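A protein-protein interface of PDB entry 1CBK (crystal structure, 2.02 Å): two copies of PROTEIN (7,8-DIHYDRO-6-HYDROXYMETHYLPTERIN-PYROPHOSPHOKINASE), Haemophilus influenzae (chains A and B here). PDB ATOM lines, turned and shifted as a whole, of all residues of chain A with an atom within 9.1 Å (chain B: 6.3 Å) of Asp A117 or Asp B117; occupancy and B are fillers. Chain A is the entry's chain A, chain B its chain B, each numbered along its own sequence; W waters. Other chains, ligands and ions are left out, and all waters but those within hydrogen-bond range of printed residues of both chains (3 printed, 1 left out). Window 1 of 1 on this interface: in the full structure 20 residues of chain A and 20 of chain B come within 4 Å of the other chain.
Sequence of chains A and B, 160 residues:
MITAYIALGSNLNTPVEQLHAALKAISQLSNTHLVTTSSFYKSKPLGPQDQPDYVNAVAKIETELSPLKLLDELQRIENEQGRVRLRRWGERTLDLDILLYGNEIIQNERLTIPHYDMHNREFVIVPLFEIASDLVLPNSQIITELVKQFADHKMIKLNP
The side-chain carboxylate (OD1) of Asp A117 lies within salt-bridge range of the guanidinium group (NH2) of Arg B121 (2.8 Å).
The guanidinium group of Arg A121 is in salt-bridge range of the side-chain carboxylate of Asp B117 (2.9 Å).
A ring nitrogen (ND1) of His A115 lies close to the backbone NH of Asp A117, at 3.4 Å.
A ring nitrogen (NE2) of His B115 sits at hydrogen-bond distance from the side-chain carboxylate (OD2) of Asp B117, at 3.4 Å.
The guanidinium group of Arg B121 is in hydrogen-bond range of the side-chain sulfur of Met B118, 3.6 Å away.
Tyr B116 touches Leu A46.
OD1 of Asp B117 touches CD2 of Leu A46, at 3.9 Å.
Leu A46 touches Asn B120.
Gly A47 touches Tyr B116.
His B115 touches Trp A89 (CD2 to CH2, 3.7 Å).
CD2 of Trp A89 touches CD1 of Tyr B116, at 3.6 Å.
Trp B89 touches Thr A112 (NE1 to CG2, 3.4 Å).
Trp B89 touches Tyr A116 (CD2 to CD2, 3.5 Å).
Asp A117 touches Leu B46.
Asp A117 touches Asp B117.
Printed residues of chain B within 4 Å of Thr A112: Trp B89 (3.4 Å).
Printed residues of chain B within 4 Å of His A115: Trp B89.
Asp A117 touches just these residues of chain B: Leu B46, Trp B89, Asp B117 and Arg B121.
Of the printed residues of chain B, Asn A120 touches Leu B46 (3.7 Å) and Asn B120 (3.6 Å).
Of chain A, only Leu A46 (3.9 Å), Trp A89 (3.8 Å), Asp A117 (3.6 Å) and Arg A121 (2.9 Å) come within 4 Å of Asp B117.
Of the printed residues of chain A, Asn B120 touches Leu A46 (3.7 Å) and Asn A120 (3.6 Å).
Printed residues of chain B that touch a printed residue of chain A: Leu B46, Trp B89, His B115, Tyr B116, Asp B117, Asn B120 and Arg B121.
Along chain A the printed residues that touch a printed residue of chain B span positions 46 to 121.
Among the printed residues, 18 pairs touch across the chains.
Among the printed residues, Asp or Glu carboxylates within 4 Å of a Lys or Arg side-chain nitrogen of the other chain: Asp A117 with Arg B121 (2.8 Å) and Arg A121 with Asp B117 (2.9 Å).
Leu A46 touches Tyr B116, but with the chains exchanged Tyr A116 does not touch Leu B46 (4.01 Å).
Leu A46 touches Asp B117, and with the chains exchanged Asp A117 touches Leu B46.
Leu A46 touches Asn B120, and with the chains exchanged Asn A120 touches Leu B46.
Asp B117 touches its own counterpart, Asp A117.
Positions printed for both chains: 46, 89, 115, 116, 117, 118, 119, 120 and 121.
Of the 18 pairs that touch across the chains among the printed residues, 14 have their exchanged pair printed and touching as well.
Water W3 lies within hydrogen-bond range of the side-chain carboxylate of Asp B117 and the guanidinium group of Arg A121.
Water W2 lies within hydrogen-bond range of OD1 of Asp B117, O of Asp A117 and ND2 of Asn B120.
Water W1 lies within hydrogen-bond range of the side-chain carboxylate of Asp A117, the side-chain amide nitrogen of Asn A120 and the backbone carbonyl oxygen of Asp B117.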
ATOM      1  N   LEU A  46     -31.641  12.205  31.452  1.00  0.00           N
ATOM      2  CA  LEU A  46     -32.169  11.851  30.145  1.00  0.00           C
ATOM      3  C   LEU A  46     -33.522  11.235  30.559  1.00  0.00           C
ATOM      4  O   LEU A  46     -33.566  10.165  31.171  1.00  0.00           O
ATOM      5  CB  LEU A  46     -31.292  10.789  29.437  1.00  0.00           C
ATOM      6  CG  LEU A  46     -31.935  10.182  28.172  1.00  0.00           C
ATOM      7  CD1 LEU A  46     -32.214  11.302  27.116  1.00  0.00           C
ATOM      8  CD2 LEU A  46     -31.031   9.087  27.605  1.00  0.00           C
ATOM      9  N   GLY A  47     -34.616  11.936  30.278  1.00  0.00           N
ATOM     10  CA  GLY A  47     -35.930  11.444  30.659  1.00  0.00           C
ATOM     11  C   GLY A  47     -36.691  12.582  31.310  1.00  0.00           C
ATOM     12  O   GLY A  47     -36.428  13.752  30.990  1.00  0.00           O
ATOM     13  N   TRP A  89     -37.713   5.527  33.297  1.00  0.00           N
ATOM     14  CA  TRP A  89     -36.979   6.731  32.913  1.00  0.00           C
ATOM     15  C   TRP A  89     -36.743   7.668  34.078  1.00  0.00           C
ATOM     16  O   TRP A  89     -36.208   8.766  33.874  1.00  0.00           O
ATOM     17  CB  TRP A  89     -37.671   7.515  31.785  1.00  0.00           C
ATOM     18  CG  TRP A  89     -37.905   6.746  30.557  1.00  0.00           C
ATOM     19  CD1 TRP A  89     -39.098   6.293  30.101  1.00  0.00           C
ATOM     20  CD2 TRP A  89     -36.928   6.372  29.580  1.00  0.00           C
ATOM     21  NE1 TRP A  89     -38.933   5.666  28.884  1.00  0.00           N
ATOM     22  CE2 TRP A  89     -37.600   5.700  28.542  1.00  0.00           C
ATOM     23  CE3 TRP A  89     -35.539   6.552  29.472  1.00  0.00           C
ATOM     24  CZ2 TRP A  89     -36.954   5.206  27.409  1.00  0.00           C
ATOM     25  CZ3 TRP A  89     -34.883   6.058  28.333  1.00  0.00           C
ATOM     26  CH2 TRP A  89     -35.598   5.395  27.321  1.00  0.00           C
ATOM     27  N   LEU A  99     -21.182  -2.311  28.677  1.00  0.00           N
ATOM     28  CA  LEU A  99     -21.133  -1.574  27.420  1.00  0.00           C
ATOM     29  C   LEU A  99     -20.435  -2.400  26.353  1.00  0.00           C
ATOM     30  O   LEU A  99     -20.913  -2.510  25.228  1.00  0.00           O
ATOM     31  CB  LEU A  99     -20.347  -0.281  27.582  1.00  0.00           C
ATOM     32  CG  LEU A  99     -20.821   0.847  28.488  1.00  0.00           C
ATOM     33  CD1 LEU A  99     -19.746   1.955  28.497  1.00  0.00           C
ATOM     34  CD2 LEU A  99     -22.156   1.404  27.961  1.00  0.00           C
ATOM     35  N   THR A 112     -27.425  -7.375  25.349  1.00  0.00           N
ATOM     36  CA  THR A 112     -27.458  -6.514  24.173  1.00  0.00           C
ATOM     37  C   THR A 112     -26.101  -5.814  24.232  1.00  0.00           C
ATOM     38  O   THR A 112     -25.974  -4.744  24.835  1.00  0.00           O
ATOM     39  CB  THR A 112     -28.562  -5.416  24.306  1.00  0.00           C
ATOM     40  OG1 THR A 112     -29.829  -6.021  24.608  1.00  0.00           O
ATOM     41  CG2 THR A 112     -28.685  -4.591  23.024  1.00  0.00           C
ATOM     42  N   PRO A 114     -22.934  -4.680  21.658  1.00  0.00           N
ATOM     43  CA  PRO A 114     -23.116  -3.333  22.224  1.00  0.00           C
ATOM     44  C   PRO A 114     -24.607  -2.937  22.275  1.00  0.00           C
ATOM     45  O   PRO A 114     -25.457  -3.602  21.690  1.00  0.00           O
ATOM     46  CB  PRO A 114     -22.410  -2.439  21.195  1.00  0.00           C
ATOM     47  CG  PRO A 114     -21.425  -3.348  20.541  1.00  0.00           C
ATOM     48  CD  PRO A 114     -22.152  -4.632  20.411  1.00  0.00           C
ATOM     49  N   HIS A 115     -24.921  -1.897  23.041  1.00  0.00           N
ATOM     50  CA  HIS A 115     -26.289  -1.365  23.071  1.00  0.00           C
ATOM     51  C   HIS A 115     -26.032   0.025  22.485  1.00  0.00           C
ATOM     52  O   HIS A 115     -25.504   0.925  23.157  1.00  0.00           O
ATOM     53  CB  HIS A 115     -26.868  -1.278  24.480  1.00  0.00           C
ATOM     54  CG  HIS A 115     -28.303  -0.844  24.505  1.00  0.00           C
ATOM     55  ND1 HIS A 115     -28.747   0.300  23.868  1.00  0.00           N
ATOM     56  CD2 HIS A 115     -29.400  -1.408  25.068  1.00  0.00           C
ATOM     57  CE1 HIS A 115     -30.052   0.416  24.036  1.00  0.00           C
ATOM     58  NE2 HIS A 115     -30.472  -0.605  24.760  1.00  0.00           N
ATOM     59  N   TYR A 116     -26.331   0.154  21.196  1.00  0.00           N
ATOM     60  CA  TYR A 116     -26.039   1.371  20.458  1.00  0.00           C
ATOM     61  C   TYR A 116     -26.640   2.660  20.895  1.00  0.00           C
ATOM     62  O   TYR A 116     -26.040   3.694  20.669  1.00  0.00           O
ATOM     63  CB  TYR A 116     -26.188   1.133  18.953  1.00  0.00           C
ATOM     64  CG  TYR A 116     -25.305  -0.015  18.472  1.00  0.00           C
ATOM     65  CD1 TYR A 116     -23.983   0.202  18.080  1.00  0.00           C
ATOM     66  CD2 TYR A 116     -25.800  -1.322  18.410  1.00  0.00           C
ATOM     67  CE1 TYR A 116     -23.177  -0.869  17.629  1.00  0.00           C
ATOM     68  CE2 TYR A 116     -24.996  -2.400  17.948  1.00  0.00           C
ATOM     69  CZ  TYR A 116     -23.700  -2.162  17.559  1.00  0.00           C
ATOM     70  OH  TYR A 116     -22.941  -3.201  17.054  1.00  0.00           O
ATOM     71  N   ASP A 117     -27.781   2.617  21.572  1.00  0.00           N
ATOM     72  CA  ASP A 117     -28.390   3.863  22.064  1.00  0.00           C
ATOM     73  C   ASP A 117     -27.481   4.527  23.089  1.00  0.00           C
ATOM     74  O   ASP A 117     -27.489   5.754  23.230  1.00  0.00           O
ATOM     75  CB  ASP A 117     -29.758   3.616  22.701  1.00  0.00           C
ATOM     76  CG  ASP A 117     -30.846   3.454  21.680  1.00  0.00           C
ATOM     77  OD1 ASP A 117     -30.834   4.197  20.663  1.00  0.00           O
ATOM     78  OD2 ASP A 117     -31.725   2.600  21.917  1.00  0.00           O
ATOM     79  N   MET A 118     -26.653   3.719  23.749  1.00  0.00           N
ATOM     80  CA  MET A 118     -25.746   4.223  24.760  1.00  0.00           C
ATOM     81  C   MET A 118     -24.576   4.992  24.173  1.00  0.00           C
ATOM     82  O   MET A 118     -24.034   5.890  24.816  1.00  0.00           O
ATOM     83  CB  MET A 118     -25.347   3.110  25.724  1.00  0.00           C
ATOM     84  CG  MET A 118     -26.593   2.605  26.464  1.00  0.00           C
ATOM     85  SD  MET A 118     -26.326   1.619  27.920  1.00  0.00           S
ATOM     86  CE  MET A 118     -25.875   2.838  29.020  1.00  0.00           C
ATOM     87  N   HIS A 119     -24.329   4.783  22.884  1.00  0.00           N
ATOM     88  CA  HIS A 119     -23.264   5.519  22.210  1.00  0.00           C
ATOM     89  C   HIS A 119     -23.735   6.928  21.851  1.00  0.00           C
ATOM     90  O   HIS A 119     -22.927   7.771  21.453  1.00  0.00           O
ATOM     91  CB  HIS A 119     -22.785   4.761  20.981  1.00  0.00           C
ATOM     92  CG  HIS A 119     -22.346   3.359  21.278  1.00  0.00           C
ATOM     93  ND1 HIS A 119     -22.055   2.447  20.287  1.00  0.00           N
ATOM     94  CD2 HIS A 119     -22.147   2.713  22.459  1.00  0.00           C
ATOM     95  CE1 HIS A 119     -21.694   1.301  20.839  1.00  0.00           C
ATOM     96  NE2 HIS A 119     -21.743   1.436  22.155  1.00  0.00           N
ATOM     97  N   ASN A 120     -25.042   7.184  22.009  1.00  0.00           N
ATOM     98  CA  ASN A 120     -25.627   8.511  21.764  1.00  0.00           C
ATOM     99  C   ASN A 120     -25.803   9.252  23.080  1.00  0.00           C
ATOM    100  O   ASN A 120     -26.382  10.336  23.116  1.00  0.00           O
ATOM    101  CB  ASN A 120     -26.982   8.382  21.064  1.00  0.00           C
ATOM    102  CG  ASN A 120     -26.843   7.959  19.607  1.00  0.00           C
ATOM    103  OD1 ASN A 120     -25.802   8.194  18.994  1.00  0.00           O
ATOM    104  ND2 ASN A 120     -27.879   7.326  19.047  1.00  0.00           N
ATOM    105  N   ARG A 121     -25.290   8.669  24.164  1.00  0.00           N
ATOM    106  CA  ARG A 121     -25.405   9.274  25.486  1.00  0.00           C
ATOM    107  C   ARG A 121     -24.109   9.939  25.898  1.00  0.00           C
ATOM    108  O   ARG A 121     -23.082   9.277  26.031  1.00  0.00           O
ATOM    109  CB  ARG A 121     -25.791   8.206  26.511  1.00  0.00           C
ATOM    110  CG  ARG A 121     -27.207   7.700  26.335  1.00  0.00           C
ATOM    111  CD  ARG A 121     -27.539   6.588  27.323  1.00  0.00           C
ATOM    112  NE  ARG A 121     -28.882   6.073  27.101  1.00  0.00           N
ATOM    113  CZ  ARG A 121     -29.551   5.316  27.959  1.00  0.00           C
ATOM    114  NH1 ARG A 121     -29.007   4.993  29.124  1.00  0.00           N
ATOM    115  NH2 ARG A 121     -30.772   4.888  27.663  1.00  0.00           N
ATOM    116  N   GLU A 122     -24.172  11.236  26.172  1.00  0.00           N
ATOM    117  CA  GLU A 122     -22.999  11.985  26.580  1.00  0.00           C
ATOM    118  C   GLU A 122     -22.337  11.447  27.852  1.00  0.00           C
ATOM    119  O   GLU A 122     -21.111  11.514  27.993  1.00  0.00           O
ATOM    120  CB  GLU A 122     -23.360  13.455  26.807  1.00  0.00           C
ATOM    121  CG  GLU A 122     -24.362  13.681  27.955  1.00  0.00           C
ATOM    122  CD  GLU A 122     -24.684  15.154  28.175  1.00  0.00           C
ATOM    123  OE1 GLU A 122     -24.073  16.027  27.514  1.00  0.00           O
ATOM    124  OE2 GLU A 122     -25.550  15.444  29.021  1.00  0.00           O
ATOM    125  N   PHE A 123     -23.158  10.974  28.786  1.00  0.00           N
ATOM    126  CA  PHE A 123     -22.668  10.476  30.067  1.00  0.00           C
ATOM    127  C   PHE A 123     -22.092   9.070  30.008  1.00  0.00           C
ATOM    128  O   PHE A 123     -21.762   8.481  31.040  1.00  0.00           O
ATOM    129  CB  PHE A 123     -23.761  10.590  31.142  1.00  0.00           C
ATOM    130  CG  PHE A 123     -25.091  10.052  30.721  1.00  0.00           C
ATOM    131  CD1 PHE A 123     -25.400   8.710  30.894  1.00  0.00           C
ATOM    132  CD2 PHE A 123     -26.052  10.898  30.184  1.00  0.00           C
ATOM    133  CE1 PHE A 123     -26.644   8.210  30.535  1.00  0.00           C
ATOM    134  CE2 PHE A 123     -27.305  10.413  29.819  1.00  0.00           C
ATOM    135  CZ  PHE A 123     -27.603   9.070  29.994  1.00  0.00           C
ATOM    136  N   VAL A 124     -22.058   8.510  28.804  1.00  0.00           N
ATOM    137  CA  VAL A 124     -21.498   7.207  28.561  1.00  0.00           C
ATOM    138  C   VAL A 124     -20.222   7.408  27.726  1.00  0.00           C
ATOM    139  O   VAL A 124     -19.130   6.953  28.107  1.00  0.00           O
ATOM    140  CB  VAL A 124     -22.458   6.322  27.763  1.00  0.00           C
ATOM    141  CG1 VAL A 124     -21.721   5.081  27.237  1.00  0.00           C
ATOM    142  CG2 VAL A 124     -23.619   5.884  28.615  1.00  0.00           C
ATOM    143  N   ILE A 125     -20.349   8.132  26.608  1.00  0.00           N
ATOM    144  CA  ILE A 125     -19.217   8.324  25.695  1.00  0.00           C
ATOM    145  C   ILE A 125     -18.094   9.218  26.177  1.00  0.00           C
ATOM    146  O   ILE A 125     -16.920   8.924  25.909  1.00  0.00           O
ATOM    147  CB  ILE A 125     -19.683   8.750  24.281  1.00  0.00           C
ATOM    148  CG1 ILE A 125     -20.528   7.632  23.654  1.00  0.00           C
ATOM    149  CG2 ILE A 125     -18.475   9.141  23.367  1.00  0.00           C
ATOM    150  CD1 ILE A 125     -19.783   6.325  23.377  1.00  0.00           C
ATOM    151  N   GLN A 149     -19.710  14.685  18.877  1.00  0.00           N
ATOM    152  CA  GLN A 149     -21.069  15.120  19.163  1.00  0.00           C
ATOM    153  C   GLN A 149     -21.237  15.731  20.570  1.00  0.00           C
ATOM    154  O   GLN A 149     -22.149  16.535  20.804  1.00  0.00           O
ATOM    155  CB  GLN A 149     -21.973  13.897  19.035  1.00  0.00           C
ATOM    156  CG  GLN A 149     -23.455  14.147  19.019  1.00  0.00           C
ATOM    157  CD  GLN A 149     -24.247  12.845  19.039  1.00  0.00           C
ATOM    158  OE1 GLN A 149     -23.689  11.748  18.902  1.00  0.00           O
ATOM    159  NE2 GLN A 149     -25.551  12.959  19.223  1.00  0.00           N
ATOM    160  N   PHE A 150     -20.350  15.366  21.494  1.00  0.00           N
ATOM    161  CA  PHE A 150     -20.438  15.825  22.871  1.00  0.00           C
ATOM    162  C   PHE A 150     -19.354  16.811  23.277  1.00  0.00           C
ATOM    163  O   PHE A 150     -19.105  17.014  24.471  1.00  0.00           O
ATOM    164  CB  PHE A 150     -20.401  14.603  23.790  1.00  0.00           C
ATOM    165  CG  PHE A 150     -21.279  13.475  23.326  1.00  0.00           C
ATOM    166  CD1 PHE A 150     -22.650  13.655  23.196  1.00  0.00           C
ATOM    167  CD2 PHE A 150     -20.727  12.226  23.010  1.00  0.00           C
ATOM    168  CE1 PHE A 150     -23.474  12.624  22.764  1.00  0.00           C
ATOM    169  CE2 PHE A 150     -21.546  11.169  22.567  1.00  0.00           C
ATOM    170  CZ  PHE A 150     -22.928  11.377  22.448  1.00  0.00           C
ATOM    171  N   LEU B  46     -27.293   3.267  12.690  1.00  0.00           N
ATOM    172  CA  LEU B  46     -27.055   3.283  14.123  1.00  0.00           C
ATOM    173  C   LEU B  46     -27.043   1.784  14.394  1.00  0.00           C
ATOM    174  O   LEU B  46     -28.071   1.125  14.312  1.00  0.00           O
ATOM    175  CB  LEU B  46     -28.210   3.936  14.893  1.00  0.00           C
ATOM    176  CG  LEU B  46     -28.051   3.893  16.424  1.00  0.00           C
ATOM    177  CD1 LEU B  46     -26.746   4.615  16.828  1.00  0.00           C
ATOM    178  CD2 LEU B  46     -29.263   4.508  17.137  1.00  0.00           C
ATOM    179  N   TRP B  89     -30.529  -4.606  15.673  1.00  0.00           N
ATOM    180  CA  TRP B  89     -29.785  -3.428  15.258  1.00  0.00           C
ATOM    181  C   TRP B  89     -29.416  -3.471  13.776  1.00  0.00           C
ATOM    182  O   TRP B  89     -28.712  -2.584  13.310  1.00  0.00           O
ATOM    183  CB  TRP B  89     -28.494  -3.276  16.079  1.00  0.00           C
ATOM    184  CG  TRP B  89     -28.688  -3.154  17.568  1.00  0.00           C
ATOM    185  CD1 TRP B  89     -28.340  -4.080  18.520  1.00  0.00           C
ATOM    186  CD2 TRP B  89     -29.185  -2.010  18.283  1.00  0.00           C
ATOM    187  NE1 TRP B  89     -28.574  -3.575  19.774  1.00  0.00           N
ATOM    188  CE2 TRP B  89     -29.091  -2.307  19.665  1.00  0.00           C
ATOM    189  CE3 TRP B  89     -29.693  -0.763  17.886  1.00  0.00           C
ATOM    190  CZ2 TRP B  89     -29.478  -1.398  20.660  1.00  0.00           C
ATOM    191  CZ3 TRP B  89     -30.083   0.147  18.875  1.00  0.00           C
ATOM    192  CH2 TRP B  89     -29.970  -0.184  20.252  1.00  0.00           C
ATOM    193  N   HIS B 115     -39.905   7.839  23.940  1.00  0.00           N
ATOM    194  CA  HIS B 115     -38.809   6.901  24.153  1.00  0.00           C
ATOM    195  C   HIS B 115     -37.627   7.848  24.071  1.00  0.00           C
ATOM    196  O   HIS B 115     -37.267   8.316  22.989  1.00  0.00           O
ATOM    197  CB  HIS B 115     -38.716   5.824  23.075  1.00  0.00           C
ATOM    198  CG  HIS B 115     -37.590   4.860  23.308  1.00  0.00           C
ATOM    199  ND1 HIS B 115     -37.762   3.488  23.286  1.00  0.00           N
ATOM    200  CD2 HIS B 115     -36.308   5.072  23.677  1.00  0.00           C
ATOM    201  CE1 HIS B 115     -36.634   2.902  23.644  1.00  0.00           C
ATOM    202  NE2 HIS B 115     -35.737   3.843  23.887  1.00  0.00           N
ATOM    203  N   TYR B 116     -37.055   8.162  25.232  1.00  0.00           N
ATOM    204  CA  TYR B 116     -35.965   9.110  25.330  1.00  0.00           C
ATOM    205  C   TYR B 116     -34.709   8.846  24.518  1.00  0.00           C
ATOM    206  O   TYR B 116     -33.990   9.784  24.186  1.00  0.00           O
ATOM    207  CB  TYR B 116     -35.666   9.438  26.795  1.00  0.00           C
ATOM    208  CG  TYR B 116     -36.828  10.171  27.444  1.00  0.00           C
ATOM    209  CD1 TYR B 116     -37.885   9.473  28.015  1.00  0.00           C
ATOM    210  CD2 TYR B 116     -36.906  11.563  27.403  1.00  0.00           C
ATOM    211  CE1 TYR B 116     -39.020  10.149  28.532  1.00  0.00           C
ATOM    212  CE2 TYR B 116     -38.024  12.248  27.918  1.00  0.00           C
ATOM    213  CZ  TYR B 116     -39.069  11.531  28.476  1.00  0.00           C
ATOM    214  OH  TYR B 116     -40.155  12.197  28.975  1.00  0.00           O
ATOM    215  N   ASP B 117     -34.464   7.602  24.128  1.00  0.00           N
ATOM    216  CA  ASP B 117     -33.260   7.358  23.328  1.00  0.00           C
ATOM    217  C   ASP B 117     -33.432   7.923  21.924  1.00  0.00           C
ATOM    218  O   ASP B 117     -32.468   8.373  21.303  1.00  0.00           O
ATOM    219  CB  ASP B 117     -32.897   5.874  23.317  1.00  0.00           C
ATOM    220  CG  ASP B 117     -32.266   5.439  24.628  1.00  0.00           C
ATOM    221  OD1 ASP B 117     -31.341   6.129  25.103  1.00  0.00           O
ATOM    222  OD2 ASP B 117     -32.689   4.401  25.164  1.00  0.00           O
ATOM    223  N   MET B 118     -34.688   8.001  21.488  1.00  0.00           N
ATOM    224  CA  MET B 118     -35.007   8.557  20.175  1.00  0.00           C
ATOM    225  C   MET B 118     -34.661  10.046  20.118  1.00  0.00           C
ATOM    226  O   MET B 118     -34.286  10.546  19.074  1.00  0.00           O
ATOM    227  CB  MET B 118     -36.477   8.337  19.842  1.00  0.00           C
ATOM    228  CG  MET B 118     -36.933   6.908  20.053  1.00  0.00           C
ATOM    229  SD  MET B 118     -36.976   5.845  18.614  1.00  0.00           S
ATOM    230  CE  MET B 118     -38.520   5.053  18.864  1.00  0.00           C
ATOM    231  N   HIS B 119     -34.691  10.732  21.256  1.00  0.00           N
ATOM    232  CA  HIS B 119     -34.353  12.160  21.295  1.00  0.00           C
ATOM    233  C   HIS B 119     -32.855  12.375  21.063  1.00  0.00           C
ATOM    234  O   HIS B 119     -32.385  13.499  20.821  1.00  0.00           O
ATOM    235  CB  HIS B 119     -34.799  12.770  22.634  1.00  0.00           C
ATOM    236  CG  HIS B 119     -36.271  12.615  22.911  1.00  0.00           C
ATOM    237  ND1 HIS B 119     -36.886  13.144  24.029  1.00  0.00           N
ATOM    238  CD2 HIS B 119     -37.253  12.007  22.199  1.00  0.00           C
ATOM    239  CE1 HIS B 119     -38.179  12.878  23.993  1.00  0.00           C
ATOM    240  NE2 HIS B 119     -38.428  12.187  22.893  1.00  0.00           N
ATOM    241  N   ASN B 120     -32.106  11.279  21.121  1.00  0.00           N
ATOM    242  CA  ASN B 120     -30.663  11.305  20.893  1.00  0.00           C
ATOM    243  C   ASN B 120     -30.274  10.891  19.462  1.00  0.00           C
ATOM    244  O   ASN B 120     -29.099  10.905  19.117  1.00  0.00           O
ATOM    245  CB  ASN B 120     -29.949  10.418  21.924  1.00  0.00           C
ATOM    246  CG  ASN B 120     -29.849  11.080  23.289  1.00  0.00           C
ATOM    247  OD1 ASN B 120     -29.794  12.306  23.380  1.00  0.00           O
ATOM    248  ND2 ASN B 120     -29.807  10.270  24.351  1.00  0.00           N
ATOM    249  N   ARG B 121     -31.269  10.574  18.627  1.00  0.00           N
ATOM    250  CA  ARG B 121     -31.037  10.165  17.238  1.00  0.00           C
ATOM    251  C   ARG B 121     -31.217  11.310  16.259  1.00  0.00           C
ATOM    252  O   ARG B 121     -32.306  11.854  16.125  1.00  0.00           O
ATOM    253  CB  ARG B 121     -31.982   9.027  16.871  1.00  0.00           C
ATOM    254  CG  ARG B 121     -31.761   7.780  17.706  1.00  0.00           C
ATOM    255  CD  ARG B 121     -32.823   6.731  17.478  1.00  0.00           C
ATOM    256  NE  ARG B 121     -32.461   5.502  18.173  1.00  0.00           N
ATOM    257  CZ  ARG B 121     -33.071   4.337  18.009  1.00  0.00           C
ATOM    258  NH1 ARG B 121     -34.100   4.222  17.177  1.00  0.00           N
ATOM    259  NH2 ARG B 121     -32.659   3.275  18.680  1.00  0.00           N
HETATM  260  O   HOH W   1     -30.166   6.884  20.629  1.00  0.00           O
HETATM  261  O   HOH W   2     -29.489   7.412  23.786  1.00  0.00           O
HETATM  262  O   HOH W   3     -32.328   2.265  26.497  1.00  0.00           O
